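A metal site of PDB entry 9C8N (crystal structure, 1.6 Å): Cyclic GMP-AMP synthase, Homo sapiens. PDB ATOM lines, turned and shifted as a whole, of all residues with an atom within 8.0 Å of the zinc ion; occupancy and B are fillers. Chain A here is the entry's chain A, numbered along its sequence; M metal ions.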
ATOM      1  N   LEU A 232     -28.947  11.791 -12.199  1.00  0.00           N
ATOM      2  CA  LEU A 232     -27.900  11.396 -11.268  1.00  0.00           C
ATOM      3  C   LEU A 232     -26.519  11.637 -11.842  1.00  0.00           C
ATOM      4  O   LEU A 232     -25.558  11.882 -11.083  1.00  0.00           O
ATOM      5  CB  LEU A 232     -28.044   9.913 -10.878  1.00  0.00           C
ATOM      6  CG  LEU A 232     -29.050   9.736  -9.750  1.00  0.00           C
ATOM      7  CD1 LEU A 232     -29.453   8.284  -9.607  1.00  0.00           C
ATOM      8  CD2 LEU A 232     -28.458  10.238  -8.385  1.00  0.00           C
ATOM      9  N   ASN A 234     -25.741  14.067 -13.871  1.00  0.00           N
ATOM     10  CA  ASN A 234     -25.546  15.506 -14.138  1.00  0.00           C
ATOM     11  C   ASN A 234     -26.389  16.216 -13.090  1.00  0.00           C
ATOM     12  O   ASN A 234     -27.453  16.765 -13.360  1.00  0.00           O
ATOM     13  CB  ASN A 234     -25.992  15.849 -15.561  1.00  0.00           C
ATOM     14  CG  ASN A 234     -25.564  17.201 -15.975  1.00  0.00           C
ATOM     15  OD1 ASN A 234     -24.947  17.973 -15.214  1.00  0.00           O
ATOM     16  ND2 ASN A 234     -25.819  17.496 -17.240  1.00  0.00           N
ATOM     17  N   HIS A 235     -25.913  16.152 -11.824  1.00  0.00           N
ATOM     18  CA  HIS A 235     -26.777  16.299 -10.674  1.00  0.00           C
ATOM     19  C   HIS A 235     -26.604  17.579  -9.883  1.00  0.00           C
ATOM     20  O   HIS A 235     -27.307  17.743  -8.884  1.00  0.00           O
ATOM     21  CB  HIS A 235     -26.546  15.106  -9.679  1.00  0.00           C
ATOM     22  CG  HIS A 235     -25.139  15.093  -9.202  1.00  0.00           C
ATOM     23  ND1 HIS A 235     -24.264  14.060  -9.484  1.00  0.00           N
ATOM     24  CD2 HIS A 235     -24.421  16.037  -8.543  1.00  0.00           C
ATOM     25  CE1 HIS A 235     -23.070  14.367  -8.984  1.00  0.00           C
ATOM     26  NE2 HIS A 235     -23.145  15.566  -8.420  1.00  0.00           N
ATOM     27  N   GLY A 236     -25.748  18.466 -10.324  1.00  0.00           N
ATOM     28  CA  GLY A 236     -25.438  19.681  -9.582  1.00  0.00           C
ATOM     29  C   GLY A 236     -26.165  20.897 -10.121  1.00  0.00           C
ATOM     30  O   GLY A 236     -26.538  20.929 -11.293  1.00  0.00           O
ATOM     31  N   LYS A 237     -26.320  21.910  -9.265  1.00  0.00           N
ATOM     32  CA  LYS A 237     -26.680  23.229  -9.801  1.00  0.00           C
ATOM     33  C   LYS A 237     -25.553  23.767 -10.673  1.00  0.00           C
ATOM     34  O   LYS A 237     -25.783  24.313 -11.760  1.00  0.00           O
ATOM     35  CB  LYS A 237     -26.960  24.223  -8.669  1.00  0.00           C
ATOM     36  CG  LYS A 237     -27.312  25.603  -9.326  1.00  0.00           C
ATOM     37  CD  LYS A 237     -27.904  26.559  -8.260  1.00  0.00           C
ATOM     38  CE  LYS A 237     -29.332  26.129  -7.858  1.00  0.00           C
ATOM     39  NZ  LYS A 237     -30.132  26.058  -9.121  1.00  0.00           N
ATOM     40  N   SER A 238     -24.308  23.637 -10.208  1.00  0.00           N
ATOM     41  CA  SER A 238     -23.176  23.949 -11.046  1.00  0.00           C
ATOM     42  C   SER A 238     -22.956  22.867 -12.097  1.00  0.00           C
ATOM     43  O   SER A 238     -22.985  21.660 -11.796  1.00  0.00           O
ATOM     44  CB  SER A 238     -21.906  24.104 -10.211  1.00  0.00           C
ATOM     45  OG  SER A 238     -20.768  24.116 -11.044  1.00  0.00           O
ATOM     46  N   THR A 240     -20.230  22.118 -13.329  1.00  0.00           N
ATOM     47  CA  THR A 240     -18.998  21.428 -13.033  1.00  0.00           C
ATOM     48  C   THR A 240     -19.046  20.694 -11.700  1.00  0.00           C
ATOM     49  O   THR A 240     -17.999  20.278 -11.220  1.00  0.00           O
ATOM     50  CB  THR A 240     -17.782  22.386 -13.107  1.00  0.00           C
ATOM     51  OG1 THR A 240     -18.044  23.626 -12.396  1.00  0.00           O
ATOM     52  CG2 THR A 240     -17.504  22.688 -14.586  1.00  0.00           C
ATOM     53  N   CYS A 241     -20.245  20.459 -11.138  1.00  0.00           N
ATOM     54  CA  CYS A 241     -20.329  19.681  -9.888  1.00  0.00           C
ATOM     55  C   CYS A 241     -19.635  18.338 -10.084  1.00  0.00           C
ATOM     56  O   CYS A 241     -19.895  17.607 -11.050  1.00  0.00           O
ATOM     57  CB  CYS A 241     -21.812  19.524  -9.505  1.00  0.00           C
ATOM     58  SG  CYS A 241     -21.982  18.955  -7.754  1.00  0.00           S
ATOM     59  N   CYS A 242     -18.744  18.038  -9.153  1.00  0.00           N
ATOM     60  CA  CYS A 242     -18.013  16.774  -9.113  1.00  0.00           C
ATOM     61  C   CYS A 242     -17.062  16.579 -10.278  1.00  0.00           C
ATOM     62  O   CYS A 242     -16.637  15.458 -10.539  1.00  0.00           O
ATOM     63  CB  CYS A 242     -18.949  15.559  -9.018  1.00  0.00           C
ATOM     64  SG  CYS A 242     -19.760  15.474  -7.371  1.00  0.00           S
ATOM     65  N   GLU A 243     -16.719  17.660 -11.010  1.00  0.00           N
ATOM     66  CA  GLU A 243     -15.680  17.591 -12.040  1.00  0.00           C
ATOM     67  C   GLU A 243     -14.348  18.108 -11.543  1.00  0.00           C
ATOM     68  O   GLU A 243     -13.347  18.021 -12.282  1.00  0.00           O
ATOM     69  CB  GLU A 243     -16.098  18.403 -13.291  1.00  0.00           C
ATOM     70  CG  GLU A 243     -17.155  17.733 -14.085  1.00  0.00           C
ATOM     71  CD  GLU A 243     -17.350  18.273 -15.485  1.00  0.00           C
ATOM     72  OE1 GLU A 243     -16.749  19.313 -15.825  1.00  0.00           O
ATOM     73  OE2 GLU A 243     -18.033  17.595 -16.245  1.00  0.00           O
ATOM     74  N   ASN A 244     -14.312  18.681 -10.347  1.00  0.00           N
ATOM     75  CA  ASN A 244     -13.054  19.146  -9.786  1.00  0.00           C
ATOM     76  C   ASN A 244     -13.072  18.989  -8.265  1.00  0.00           C
ATOM     77  O   ASN A 244     -14.134  18.820  -7.649  1.00  0.00           O
ATOM     78  CB  ASN A 244     -12.800  20.592 -10.206  1.00  0.00           C
ATOM     79  CG  ASN A 244     -13.897  21.532  -9.764  1.00  0.00           C
ATOM     80  OD1 ASN A 244     -14.009  21.813  -8.595  1.00  0.00           O
ATOM     81  ND2 ASN A 244     -14.698  22.039 -10.715  1.00  0.00           N
ATOM     82  N   GLU A 247     -15.494  20.956  -6.012  1.00  0.00           N
ATOM     83  CA  GLU A 247     -16.929  20.742  -6.165  1.00  0.00           C
ATOM     84  C   GLU A 247     -17.290  19.264  -6.034  1.00  0.00           C
ATOM     85  O   GLU A 247     -18.189  18.770  -6.691  1.00  0.00           O
ATOM     86  CB  GLU A 247     -17.433  21.264  -7.519  1.00  0.00           C
ATOM     87  CG  GLU A 247     -17.239  22.759  -7.734  1.00  0.00           C
ATOM     88  CD  GLU A 247     -17.818  23.258  -9.043  1.00  0.00           C
ATOM     89  OE1 GLU A 247     -19.058  23.326  -9.181  1.00  0.00           O
ATOM     90  OE2 GLU A 247     -17.036  23.654  -9.926  1.00  0.00           O
ATOM     91  N   LYS A 248     -16.657  18.538  -5.112  1.00  0.00           N
ATOM     92  CA  LYS A 248     -16.993  17.127  -4.922  1.00  0.00           C
ATOM     93  C   LYS A 248     -18.133  17.034  -3.897  1.00  0.00           C
ATOM     94  O   LYS A 248     -17.903  16.837  -2.699  1.00  0.00           O
ATOM     95  CB  LYS A 248     -15.764  16.344  -4.462  1.00  0.00           C
ATOM     96  CG  LYS A 248     -14.753  16.180  -5.557  1.00  0.00           C
ATOM     97  CD  LYS A 248     -15.103  15.029  -6.489  1.00  0.00           C
ATOM     98  CE  LYS A 248     -14.340  15.100  -7.818  1.00  0.00           C
ATOM     99  NZ  LYS A 248     -14.406  13.762  -8.487  1.00  0.00           N
ATOM    100  N   CYS A 249     -19.382  17.135  -4.367  1.00  0.00           N
ATOM    101  CA  CYS A 249     -20.504  17.144  -3.441  1.00  0.00           C
ATOM    102  C   CYS A 249     -20.742  15.732  -2.898  1.00  0.00           C
ATOM    103  O   CYS A 249     -20.138  14.743  -3.342  1.00  0.00           O
ATOM    104  CB  CYS A 249     -21.771  17.685  -4.130  1.00  0.00           C
ATOM    105  SG  CYS A 249     -22.677  16.496  -5.185  1.00  0.00           S
ATOM    106  N   CYS A 250     -21.646  15.646  -1.920  1.00  0.00           N
ATOM    107  CA  CYS A 250     -21.935  14.355  -1.298  1.00  0.00           C
ATOM    108  C   CYS A 250     -23.300  13.797  -1.642  1.00  0.00           C
ATOM    109  O   CYS A 250     -23.822  12.915  -0.933  1.00  0.00           O
ATOM    110  CB  CYS A 250     -21.797  14.470   0.247  1.00  0.00           C
ATOM    111  SG  CYS A 250     -23.032  15.429   1.122  1.00  0.00           S
ATOM    112  N   ARG A 251     -23.889  14.219  -2.771  1.00  0.00           N
ATOM    113  CA  ARG A 251     -25.199  13.684  -3.152  1.00  0.00           C
ATOM    114  C   ARG A 251     -25.133  12.161  -3.348  1.00  0.00           C
ATOM    115  O   ARG A 251     -25.950  11.416  -2.777  1.00  0.00           O
ATOM    116  CB  ARG A 251     -25.701  14.383  -4.447  1.00  0.00           C
ATOM    117  CG  ARG A 251     -26.194  15.800  -4.190  1.00  0.00           C
ATOM    118  CD  ARG A 251     -26.829  16.404  -5.458  1.00  0.00           C
ATOM    119  NE  ARG A 251     -27.293  17.790  -5.331  1.00  0.00           N
ATOM    120  CZ  ARG A 251     -26.526  18.843  -5.607  1.00  0.00           C
ATOM    121  NH1 ARG A 251     -25.238  18.708  -5.897  1.00  0.00           N
ATOM    122  NH2 ARG A 251     -27.100  20.048  -5.720  1.00  0.00           N
ATOM    123  N   LYS A 252     -24.225  11.689  -4.225  1.00  0.00           N
ATOM    124  CA  LYS A 252     -24.201  10.250  -4.524  1.00  0.00           C
ATOM    125  C   LYS A 252     -23.807   9.440  -3.289  1.00  0.00           C
ATOM    126  O   LYS A 252     -24.351   8.366  -3.075  1.00  0.00           O
ATOM    127  CB  LYS A 252     -23.235   9.947  -5.699  1.00  0.00           C
ATOM    128  CG  LYS A 252     -23.860  10.358  -7.020  1.00  0.00           C
ATOM    129  CD  LYS A 252     -23.106   9.741  -8.196  1.00  0.00           C
ATOM    130  CE  LYS A 252     -23.758  10.253  -9.473  1.00  0.00           C
ATOM    131  NZ  LYS A 252     -23.207   9.599 -10.708  1.00  0.00           N
ATOM    132  N   ASP A 297     -25.720  23.404  -4.336  1.00  0.00           N
ATOM    133  CA  ASP A 297     -24.590  22.503  -4.138  1.00  0.00           C
ATOM    134  C   ASP A 297     -23.999  22.696  -2.746  1.00  0.00           C
ATOM    135  O   ASP A 297     -23.483  21.740  -2.144  1.00  0.00           O
ATOM    136  CB  ASP A 297     -23.505  22.680  -5.209  1.00  0.00           C
ATOM    137  CG  ASP A 297     -23.996  22.387  -6.612  1.00  0.00           C
ATOM    138  OD1 ASP A 297     -24.964  21.623  -6.749  1.00  0.00           O
ATOM    139  OD2 ASP A 297     -23.408  22.956  -7.557  1.00  0.00           O
ATOM    140  N   TRP A 300     -24.865  20.280   0.014  1.00  0.00           N
ATOM    141  CA  TRP A 300     -24.344  18.934  -0.213  1.00  0.00           C
ATOM    142  C   TRP A 300     -22.823  18.953  -0.155  1.00  0.00           C
ATOM    143  O   TRP A 300     -22.144  18.201  -0.847  1.00  0.00           O
ATOM    144  CB  TRP A 300     -24.842  18.364  -1.557  1.00  0.00           C
ATOM    145  CG  TRP A 300     -26.314  18.256  -1.601  1.00  0.00           C
ATOM    146  CD1 TRP A 300     -27.233  19.165  -2.127  1.00  0.00           C
ATOM    147  CD2 TRP A 300     -27.113  17.195  -1.055  1.00  0.00           C
ATOM    148  NE1 TRP A 300     -28.502  18.745  -1.920  1.00  0.00           N
ATOM    149  CE2 TRP A 300     -28.466  17.492  -1.325  1.00  0.00           C
ATOM    150  CE3 TRP A 300     -26.804  15.968  -0.421  1.00  0.00           C
ATOM    151  CZ2 TRP A 300     -29.512  16.655  -0.980  1.00  0.00           C
ATOM    152  CZ3 TRP A 300     -27.876  15.109  -0.052  1.00  0.00           C
ATOM    153  CH2 TRP A 300     -29.210  15.449  -0.344  1.00  0.00           C
HETATM  154 ZN    ZN M   1     -21.700  16.703  -7.379  1.00  0.00          ZN
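The guanidinium group (NH1) of Arg 251 sits close to the side-chain sulfur (SG) of Cys 241, at 3.8 Å.
The backbone NH of Cys 242 lies within hydrogen-bond range of the backbone carbonyl oxygen of Glu 247.
The backbone carbonyl oxygen of Leu 232 is in hydrogen-bond range of a ring nitrogen (ND1) of His 235.
NH1 of Arg 251 sits close to SG of Cys 249 (3.5 Å).
The side-chain amino group (NZ) of Lys 248 is in hydrogen-bond range of the backbone carbonyl oxygen (O) of Cys 242, at 3.5 Å.
Along chain A the residues within 4 Å of the zinc ion span positions 235 to 249.
A ring nitrogen (NE2) of His 235 binds the zinc ion.
The zinc ion is bound by the side-chain sulfur (SG) of Cys 242, 2.3 Å away.
The zinc ion is bound by SG of Cys 241, 2.3 Å away.
SG of Cys 249 binds the zinc ion (2.4 Å).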
